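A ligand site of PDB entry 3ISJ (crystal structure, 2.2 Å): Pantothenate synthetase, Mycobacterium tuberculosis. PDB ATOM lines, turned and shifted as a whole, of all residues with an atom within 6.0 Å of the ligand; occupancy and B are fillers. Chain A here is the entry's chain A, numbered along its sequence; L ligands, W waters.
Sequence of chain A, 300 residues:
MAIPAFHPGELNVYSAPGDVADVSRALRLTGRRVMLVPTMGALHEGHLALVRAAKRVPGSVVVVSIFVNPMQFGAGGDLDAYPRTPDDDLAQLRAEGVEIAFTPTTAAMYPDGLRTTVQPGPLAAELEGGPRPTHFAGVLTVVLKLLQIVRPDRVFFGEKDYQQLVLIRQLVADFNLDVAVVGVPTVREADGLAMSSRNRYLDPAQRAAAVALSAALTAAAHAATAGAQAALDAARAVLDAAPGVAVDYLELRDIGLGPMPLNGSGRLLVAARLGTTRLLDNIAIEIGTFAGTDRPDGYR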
ATOM      1  N   PRO A  38     -27.773 -16.443  -4.731  1.00  0.00           N
ATOM      2  CA  PRO A  38     -27.517 -17.325  -3.586  1.00  0.00           C
ATOM      3  C   PRO A  38     -27.268 -16.553  -2.353  1.00  0.00           C
ATOM      4  O   PRO A  38     -26.347 -15.776  -2.319  1.00  0.00           O
ATOM      5  CB  PRO A  38     -26.234 -17.987  -3.971  1.00  0.00           C
ATOM      6  CG  PRO A  38     -26.158 -17.820  -5.451  1.00  0.00           C
ATOM      7  CD  PRO A  38     -26.649 -16.491  -5.685  1.00  0.00           C
ATOM      8  N   THR A  39     -28.131 -16.733  -1.358  1.00  0.00           N
ATOM      9  CA  THR A  39     -27.953 -16.076  -0.072  1.00  0.00           C
ATOM     10  C   THR A  39     -27.945 -17.101   1.090  1.00  0.00           C
ATOM     11  O   THR A  39     -28.398 -18.252   0.924  1.00  0.00           O
ATOM     12  CB  THR A  39     -29.073 -14.964   0.150  1.00  0.00           C
ATOM     13  OG1 THR A  39     -30.301 -15.549   0.597  1.00  0.00           O
ATOM     14  CG2 THR A  39     -29.344 -14.241  -1.162  1.00  0.00           C
ATOM     15  N   MET A  40     -27.413 -16.700   2.225  1.00  0.00           N
ATOM     16  CA  MET A  40     -27.620 -17.419   3.448  1.00  0.00           C
ATOM     17  C   MET A  40     -28.752 -16.798   4.282  1.00  0.00           C
ATOM     18  O   MET A  40     -28.785 -16.958   5.507  1.00  0.00           O
ATOM     19  CB  MET A  40     -26.307 -17.534   4.227  1.00  0.00           C
ATOM     20  CG  MET A  40     -25.239 -18.351   3.495  1.00  0.00           C
ATOM     21  SD  MET A  40     -23.971 -19.075   4.585  1.00  0.00           S
ATOM     22  CE  MET A  40     -23.074 -17.535   4.893  1.00  0.00           C
ATOM     23  N   GLY A  41     -29.700 -16.138   3.623  1.00  0.00           N
ATOM     24  CA  GLY A  41     -30.742 -15.343   4.342  1.00  0.00           C
ATOM     25  C   GLY A  41     -30.249 -14.126   5.192  1.00  0.00           C
ATOM     26  O   GLY A  41     -29.122 -13.625   5.025  1.00  0.00           O
ATOM     27  N   HIS A  44     -30.236  -8.059   3.691  1.00  0.00           N
ATOM     28  CA  HIS A  44     -30.115  -6.655   3.962  1.00  0.00           C
ATOM     29  C   HIS A  44     -30.102  -5.972   2.598  1.00  0.00           C
ATOM     30  O   HIS A  44     -30.177  -6.626   1.542  1.00  0.00           O
ATOM     31  CB  HIS A  44     -28.858  -6.365   4.771  1.00  0.00           C
ATOM     32  CG  HIS A  44     -27.652  -7.112   4.286  1.00  0.00           C
ATOM     33  ND1 HIS A  44     -27.002  -6.775   3.111  1.00  0.00           N
ATOM     34  CD2 HIS A  44     -27.035  -8.219   4.746  1.00  0.00           C
ATOM     35  CE1 HIS A  44     -26.012  -7.628   2.906  1.00  0.00           C
ATOM     36  NE2 HIS A  44     -26.024  -8.521   3.871  1.00  0.00           N
ATOM     37  N   GLU A  45     -29.986  -4.657   2.645  1.00  0.00           N
ATOM     38  CA  GLU A  45     -29.950  -3.835   1.466  1.00  0.00           C
ATOM     39  C   GLU A  45     -28.910  -4.369   0.435  1.00  0.00           C
ATOM     40  O   GLU A  45     -29.180  -4.368  -0.793  1.00  0.00           O
ATOM     41  CB  GLU A  45     -29.733  -2.378   1.925  1.00  0.00           C
ATOM     42  CG  GLU A  45     -29.967  -1.297   0.887  1.00  0.00           C
ATOM     43  CD  GLU A  45     -31.356  -1.347   0.251  1.00  0.00           C
ATOM     44  OE1 GLU A  45     -32.366  -1.667   0.946  1.00  0.00           O
ATOM     45  OE2 GLU A  45     -31.411  -1.030  -0.947  1.00  0.00           O
ATOM     46  N   GLY A  46     -27.780  -4.892   0.920  1.00  0.00           N
ATOM     47  CA  GLY A  46     -26.758  -5.545   0.050  1.00  0.00           C
ATOM     48  C   GLY A  46     -27.327  -6.676  -0.782  1.00  0.00           C
ATOM     49  O   GLY A  46     -27.221  -6.692  -2.038  1.00  0.00           O
ATOM     50  N   HIS A  47     -27.981  -7.613  -0.117  1.00  0.00           N
ATOM     51  CA  HIS A  47     -28.849  -8.592  -0.831  1.00  0.00           C
ATOM     52  C   HIS A  47     -29.828  -8.020  -1.834  1.00  0.00           C
ATOM     53  O   HIS A  47     -29.978  -8.599  -2.896  1.00  0.00           O
ATOM     54  CB  HIS A  47     -29.622  -9.471   0.152  1.00  0.00           C
ATOM     55  CG  HIS A  47     -28.728 -10.378   0.895  1.00  0.00           C
ATOM     56  ND1 HIS A  47     -28.508 -10.246   2.251  1.00  0.00           N
ATOM     57  CD2 HIS A  47     -27.932 -11.387   0.479  1.00  0.00           C
ATOM     58  CE1 HIS A  47     -27.658 -11.179   2.636  1.00  0.00           C
ATOM     59  NE2 HIS A  47     -27.269 -11.857   1.574  1.00  0.00           N
ATOM     60  N   ALA A  49     -29.764  -5.214  -3.490  1.00  0.00           N
ATOM     61  CA  ALA A  49     -29.038  -4.703  -4.652  1.00  0.00           C
ATOM     62  C   ALA A  49     -28.788  -5.812  -5.639  1.00  0.00           C
ATOM     63  O   ALA A  49     -28.881  -5.593  -6.856  1.00  0.00           O
ATOM     64  CB  ALA A  49     -27.677  -4.059  -4.226  1.00  0.00           C
ATOM     65  N   LEU A  50     -28.473  -6.998  -5.124  1.00  0.00           N
ATOM     66  CA  LEU A  50     -28.225  -8.188  -5.969  1.00  0.00           C
ATOM     67  C   LEU A  50     -29.535  -8.524  -6.654  1.00  0.00           C
ATOM     68  O   LEU A  50     -29.566  -8.751  -7.839  1.00  0.00           O
ATOM     69  CB  LEU A  50     -27.759  -9.365  -5.081  1.00  0.00           C
ATOM     70  CG  LEU A  50     -26.454  -9.289  -4.259  1.00  0.00           C
ATOM     71  CD1 LEU A  50     -26.171 -10.674  -3.645  1.00  0.00           C
ATOM     72  CD2 LEU A  50     -25.222  -8.814  -5.113  1.00  0.00           C
ATOM     73  N   GLN A  72     -19.482 -24.879   4.802  1.00  0.00           N
ATOM     74  CA  GLN A  72     -18.531 -23.754   4.779  1.00  0.00           C
ATOM     75  C   GLN A  72     -18.281 -23.183   6.225  1.00  0.00           C
ATOM     76  O   GLN A  72     -17.500 -22.216   6.424  1.00  0.00           O
ATOM     77  CB  GLN A  72     -19.028 -22.695   3.824  1.00  0.00           C
ATOM     78  CG  GLN A  72     -20.366 -22.058   4.236  1.00  0.00           C
ATOM     79  CD  GLN A  72     -20.946 -21.113   3.195  1.00  0.00           C
ATOM     80  OE1 GLN A  72     -20.860 -19.896   3.331  1.00  0.00           O
ATOM     81  NE2 GLN A  72     -21.512 -21.672   2.126  1.00  0.00           N
ATOM     82  N   TYR A  82     -25.096 -17.875  13.148  1.00  0.00           N
ATOM     83  CA  TYR A  82     -25.647 -17.242  11.937  1.00  0.00           C
ATOM     84  C   TYR A  82     -27.126 -16.846  11.963  1.00  0.00           C
ATOM     85  O   TYR A  82     -27.979 -17.737  12.082  1.00  0.00           O
ATOM     86  CB  TYR A  82     -25.404 -18.099  10.694  1.00  0.00           C
ATOM     87  CG  TYR A  82     -25.452 -17.252   9.456  1.00  0.00           C
ATOM     88  CD1 TYR A  82     -24.291 -16.602   9.000  1.00  0.00           C
ATOM     89  CD2 TYR A  82     -26.651 -17.025   8.782  1.00  0.00           C
ATOM     90  CE1 TYR A  82     -24.313 -15.767   7.882  1.00  0.00           C
ATOM     91  CE2 TYR A  82     -26.686 -16.189   7.638  1.00  0.00           C
ATOM     92  CZ  TYR A  82     -25.492 -15.571   7.208  1.00  0.00           C
ATOM     93  OH  TYR A  82     -25.476 -14.769   6.105  1.00  0.00           O
ATOM     94  N   PHE A 157     -23.285 -12.218  -7.268  1.00  0.00           N
ATOM     95  CA  PHE A 157     -22.661 -12.094  -5.953  1.00  0.00           C
ATOM     96  C   PHE A 157     -22.184 -10.655  -5.622  1.00  0.00           C
ATOM     97  O   PHE A 157     -21.891  -9.902  -6.518  1.00  0.00           O
ATOM     98  CB  PHE A 157     -21.455 -13.032  -5.932  1.00  0.00           C
ATOM     99  CG  PHE A 157     -21.821 -14.500  -5.851  1.00  0.00           C
ATOM    100  CD1 PHE A 157     -22.189 -15.087  -4.611  1.00  0.00           C
ATOM    101  CD2 PHE A 157     -21.847 -15.298  -7.037  1.00  0.00           C
ATOM    102  CE1 PHE A 157     -22.484 -16.450  -4.539  1.00  0.00           C
ATOM    103  CE2 PHE A 157     -22.182 -16.648  -6.979  1.00  0.00           C
ATOM    104  CZ  PHE A 157     -22.492 -17.229  -5.711  1.00  0.00           C
ATOM    105  N   GLY A 158     -22.091 -10.302  -4.350  1.00  0.00           N
ATOM    106  CA  GLY A 158     -21.438  -9.086  -3.947  1.00  0.00           C
ATOM    107  C   GLY A 158     -19.927  -9.094  -4.097  1.00  0.00           C
ATOM    108  O   GLY A 158     -19.308 -10.170  -4.184  1.00  0.00           O
ATOM    109  N   GLU A 159     -19.304  -7.915  -4.092  1.00  0.00           N
ATOM    110  CA  GLU A 159     -17.839  -7.849  -4.006  1.00  0.00           C
ATOM    111  C   GLU A 159     -17.448  -7.709  -2.576  1.00  0.00           C
ATOM    112  O   GLU A 159     -16.274  -7.623  -2.246  1.00  0.00           O
ATOM    113  CB  GLU A 159     -17.262  -6.696  -4.837  1.00  0.00           C
ATOM    114  CG  GLU A 159     -17.816  -6.614  -6.267  1.00  0.00           C
ATOM    115  CD  GLU A 159     -17.329  -5.325  -7.005  1.00  0.00           C
ATOM    116  OE1 GLU A 159     -17.071  -4.291  -6.336  1.00  0.00           O
ATOM    117  OE2 GLU A 159     -17.237  -5.349  -8.243  1.00  0.00           O
ATOM    118  N   LYS A 160     -18.430  -7.690  -1.693  1.00  0.00           N
ATOM    119  CA  LYS A 160     -18.102  -7.736  -0.295  1.00  0.00           C
ATOM    120  C   LYS A 160     -17.248  -9.000  -0.103  1.00  0.00           C
ATOM    121  O   LYS A 160     -16.104  -8.953   0.397  1.00  0.00           O
ATOM    122  CB  LYS A 160     -19.386  -7.746   0.523  1.00  0.00           C
ATOM    123  CG  LYS A 160     -19.309  -7.162   1.955  1.00  0.00           C
ATOM    124  CD  LYS A 160     -18.017  -7.446   2.693  1.00  0.00           C
ATOM    125  CE  LYS A 160     -18.306  -7.588   4.167  1.00  0.00           C
ATOM    126  NZ  LYS A 160     -19.588  -6.875   4.387  1.00  0.00           N
ATOM    127  N   ASP A 161     -17.777 -10.165  -0.510  1.00  0.00           N
ATOM    128  CA  ASP A 161     -16.974 -11.346  -0.368  1.00  0.00           C
ATOM    129  C   ASP A 161     -16.211 -11.578  -1.642  1.00  0.00           C
ATOM    130  O   ASP A 161     -16.613 -12.340  -2.531  1.00  0.00           O
ATOM    131  CB  ASP A 161     -17.843 -12.487   0.095  1.00  0.00           C
ATOM    132  CG  ASP A 161     -18.585 -12.136   1.418  1.00  0.00           C
ATOM    133  OD1 ASP A 161     -17.911 -12.085   2.461  1.00  0.00           O
ATOM    134  OD2 ASP A 161     -19.811 -11.848   1.428  1.00  0.00           O
ATOM    135  N   GLN A 164     -14.346 -15.039  -2.348  1.00  0.00           N
ATOM    136  CA  GLN A 164     -15.355 -15.959  -2.723  1.00  0.00           C
ATOM    137  C   GLN A 164     -15.784 -15.766  -4.188  1.00  0.00           C
ATOM    138  O   GLN A 164     -15.994 -16.762  -4.924  1.00  0.00           O
ATOM    139  CB  GLN A 164     -16.523 -15.656  -1.849  1.00  0.00           C
ATOM    140  CG  GLN A 164     -17.699 -16.514  -2.118  1.00  0.00           C
ATOM    141  CD  GLN A 164     -18.839 -16.194  -1.213  1.00  0.00           C
ATOM    142  OE1 GLN A 164     -18.898 -16.662  -0.087  1.00  0.00           O
ATOM    143  NE2 GLN A 164     -19.739 -15.347  -1.688  1.00  0.00           N
ATOM    144  N   VAL A 184     -21.425  -7.537  -8.019  1.00  0.00           N
ATOM    145  CA  VAL A 184     -22.195  -6.299  -7.831  1.00  0.00           C
ATOM    146  C   VAL A 184     -21.498  -5.479  -6.738  1.00  0.00           C
ATOM    147  O   VAL A 184     -21.217  -6.022  -5.637  1.00  0.00           O
ATOM    148  CB  VAL A 184     -23.633  -6.629  -7.394  1.00  0.00           C
ATOM    149  CG1 VAL A 184     -24.418  -5.340  -7.062  1.00  0.00           C
ATOM    150  CG2 VAL A 184     -24.334  -7.379  -8.459  1.00  0.00           C
ATOM    151  N   PRO A 185     -21.156  -4.179  -7.048  1.00  0.00           N
ATOM    152  CA  PRO A 185     -20.422  -3.341  -6.062  1.00  0.00           C
ATOM    153  C   PRO A 185     -21.084  -3.326  -4.690  1.00  0.00           C
ATOM    154  O   PRO A 185     -22.305  -3.329  -4.604  1.00  0.00           O
ATOM    155  CB  PRO A 185     -20.443  -1.945  -6.714  1.00  0.00           C
ATOM    156  CG  PRO A 185     -20.388  -2.247  -8.167  1.00  0.00           C
ATOM    157  CD  PRO A 185     -21.394  -3.418  -8.296  1.00  0.00           C
ATOM    158  N   THR A 186     -20.274  -3.305  -3.637  1.00  0.00           N
ATOM    159  CA  THR A 186     -20.684  -3.448  -2.250  1.00  0.00           C
ATOM    160  C   THR A 186     -21.559  -2.284  -1.812  1.00  0.00           C
ATOM    161  O   THR A 186     -21.196  -1.116  -2.036  1.00  0.00           O
ATOM    162  CB  THR A 186     -19.395  -3.471  -1.422  1.00  0.00           C
ATOM    163  OG1 THR A 186     -18.503  -4.467  -1.963  1.00  0.00           O
ATOM    164  CG2 THR A 186     -19.615  -3.709   0.047  1.00  0.00           C
ATOM    165  N   VAL A 187     -22.701  -2.594  -1.207  1.00  0.00           N
ATOM    166  CA  VAL A 187     -23.664  -1.594  -0.765  1.00  0.00           C
ATOM    167  C   VAL A 187     -23.149  -1.222   0.589  1.00  0.00           C
ATOM    168  O   VAL A 187     -22.660  -2.090   1.321  1.00  0.00           O
ATOM    169  CB  VAL A 187     -25.074  -2.165  -0.574  1.00  0.00           C
ATOM    170  CG1 VAL A 187     -25.957  -1.151   0.141  1.00  0.00           C
ATOM    171  CG2 VAL A 187     -25.686  -2.571  -1.894  1.00  0.00           C
ATOM    172  N   ALA A 194     -19.447  -1.322   5.078  1.00  0.00           N
ATOM    173  CA  ALA A 194     -19.900  -2.291   4.094  1.00  0.00           C
ATOM    174  C   ALA A 194     -21.017  -3.054   4.748  1.00  0.00           C
ATOM    175  O   ALA A 194     -20.859  -3.499   5.857  1.00  0.00           O
ATOM    176  CB  ALA A 194     -18.761  -3.204   3.748  1.00  0.00           C
ATOM    177  N   MET A 195     -22.158  -3.152   4.078  1.00  0.00           N
ATOM    178  CA  MET A 195     -23.271  -4.006   4.526  1.00  0.00           C
ATOM    179  C   MET A 195     -22.846  -5.430   4.889  1.00  0.00           C
ATOM    180  O   MET A 195     -22.076  -6.076   4.165  1.00  0.00           O
ATOM    181  CB  MET A 195     -24.325  -4.110   3.445  1.00  0.00           C
ATOM    182  CG  MET A 195     -25.108  -2.850   3.284  1.00  0.00           C
ATOM    183  SD  MET A 195     -26.076  -2.513   4.740  1.00  0.00           S
ATOM    184  CE  MET A 195     -26.845  -0.963   4.160  1.00  0.00           C
ATOM    185  N   SER A 196     -23.342  -5.918   6.017  1.00  0.00           N
ATOM    186  CA  SER A 196     -23.032  -7.254   6.474  1.00  0.00           C
ATOM    187  C   SER A 196     -24.080  -7.572   7.522  1.00  0.00           C
ATOM    188  O   SER A 196     -24.463  -6.704   8.320  1.00  0.00           O
ATOM    189  CB  SER A 196     -21.636  -7.295   7.114  1.00  0.00           C
ATOM    190  OG  SER A 196     -21.278  -8.574   7.616  1.00  0.00           O
ATOM    191  N   SER A 197     -24.511  -8.835   7.508  1.00  0.00           N
ATOM    192  CA  SER A 197     -25.321  -9.410   8.575  1.00  0.00           C
ATOM    193  C   SER A 197     -24.547  -9.377   9.891  1.00  0.00           C
ATOM    194  O   SER A 197     -25.149  -9.155  10.952  1.00  0.00           O
ATOM    195  CB  SER A 197     -25.713 -10.845   8.214  1.00  0.00           C
ATOM    196  OG  SER A 197     -24.539 -11.640   7.943  1.00  0.00           O
HETATM  197  C1  LIG L   1     -24.156  -5.575  -3.143  1.00  0.00           C
HETATM  198  C2  LIG L   1     -24.306 -15.515   0.177  1.00  0.00           C
HETATM  199  O1  LIG L   1     -23.585 -11.932   3.030  1.00  0.00           O
HETATM  200  O2  LIG L   1     -23.090 -14.723   2.418  1.00  0.00           O
HETATM  201  O3  LIG L   1     -25.521 -14.359   2.442  1.00  0.00           O
HETATM  202  C3  LIG L   1     -23.110  -6.096   0.392  1.00  0.00           C
HETATM  203  C4  LIG L   1     -23.011  -7.058   1.411  1.00  0.00           C
HETATM  204  C5  LIG L   1     -23.769  -7.872  -1.121  1.00  0.00           C
HETATM  205  C6  LIG L   1     -23.855 -10.093  -0.002  1.00  0.00           C
HETATM  206  N1  LIG L   1     -24.038 -12.768   0.938  1.00  0.00           N
HETATM  207  N2  LIG L   1     -23.249  -9.397   1.989  1.00  0.00           N
HETATM  208  O4  LIG L   1     -23.527  -5.492  -1.833  1.00  0.00           O
HETATM  209  C7  LIG L   1     -23.721 -11.750   1.800  1.00  0.00           C
HETATM  210  C8  LIG L   1     -23.497  -6.488  -0.904  1.00  0.00           C
HETATM  211  C9  LIG L   1     -23.613 -10.483   1.269  1.00  0.00           C
HETATM  212  C10 LIG L   1     -23.634  -8.765  -0.084  1.00  0.00           C
HETATM  213  C11 LIG L   1     -23.271  -8.342   1.158  1.00  0.00           C
HETATM  214  S1  LIG L   1     -24.258 -14.398   1.565  1.00  0.00           S
HETATM  215  O   HOH W   1     -23.162 -12.675  -2.442  1.00  0.00           O
HETATM  216  O   HOH W   2     -21.418 -10.314   4.590  1.00  0.00           O
HETATM  217  O   HOH W   3     -24.393 -10.433   5.119  1.00  0.00           O
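Residues that only touch the ligand: Met 195 (3.1 Å), Pro 38 (3.2 Å), Pro 185 (3.3 Å), Gly 46 (3.4 Å), Thr 186 (3.5 Å), Tyr 82 (3.7 Å), Thr 39 (3.7 Å), Lys 160 (3.7 Å), Gly 158 (3.9 Å), Val 184 (3.9 Å), Asp 161 (3.9 Å), Leu 50 (3.9 Å) and Ala 49 (3.98 Å).
Hydrophobic or aromatic side chains that line the ligand: Met 40, His 44, His 47, Ala 49, Leu 50, Val 184, Val 187 and Met 195.
Within 4 Å of the ligand: Pro 38, Thr 39, Met 40, His 44, Gly 46, His 47, Ala 49, Leu 50, Tyr 82, Gly 158, Lys 160, Asp 161, Val 184, Pro 185, Thr 186, Val 187 and Met 195.
The nearest printed residue that does not touch the ligand is Gly 41 (4.5 Å).
Water W3 lies within hydrogen-bond range of O1 of the ligand (2.7 Å), NE2 of His 44 (2.8 Å) and N of Ser 197 (2.9 Å).
Water W2 bridges an oxygen (O1) of the ligand (3.1 Å) and the side-chain hydroxyl of Ser 196 (3.5 Å).
Water W1 bridges N of Gly 158 (3.2 Å) and N1 of the ligand (3.5 Å).
OG1 of Thr 39 sits at hydrogen-bond distance from N of Gly 41 (3.1 Å).
The backbone NH of Val 184 sits at hydrogen-bond distance from the backbone carbonyl oxygen of Phe 157, at 2.8 Å.
The side-chain hydroxyl (OG1) of Thr 186 sits at hydrogen-bond distance from the backbone NH (N) of Lys 160 (3.2 Å).
The side-chain amino group (NZ) of Lys 160 is in hydrogen-bond range of the backbone carbonyl oxygen (O) of Met 195.
The backbone carbonyl oxygen (O) of Val 184 sits at hydrogen-bond distance from the backbone NH (N) of Glu 159.
A ring nitrogen (ND1) of His 47 lies within hydrogen-bond range of the backbone NH (N) of His 44 (3.1 Å).
A ring nitrogen (ND1) of His 44 sits at hydrogen-bond distance from the backbone NH (N) of Gly 46 (3.0 Å).
SD of Met 40 lies close to OE1 of Gln 72, 3.5 Å away.
A nitrogen (N2) of the ligand sits close to a ring nitrogen (NE2) of His 44.
NE2 of His 47 sits at hydrogen-bond distance from O3 of the ligand (3.2 Å).
The backbone NH (N) of Val 187 is in hydrogen-bond range of an oxygen (O4) of the ligand, 3.1 Å away.
An oxygen (O3) of the ligand lies within hydrogen-bond range of the backbone NH (N) of Met 40 (3.0 Å).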
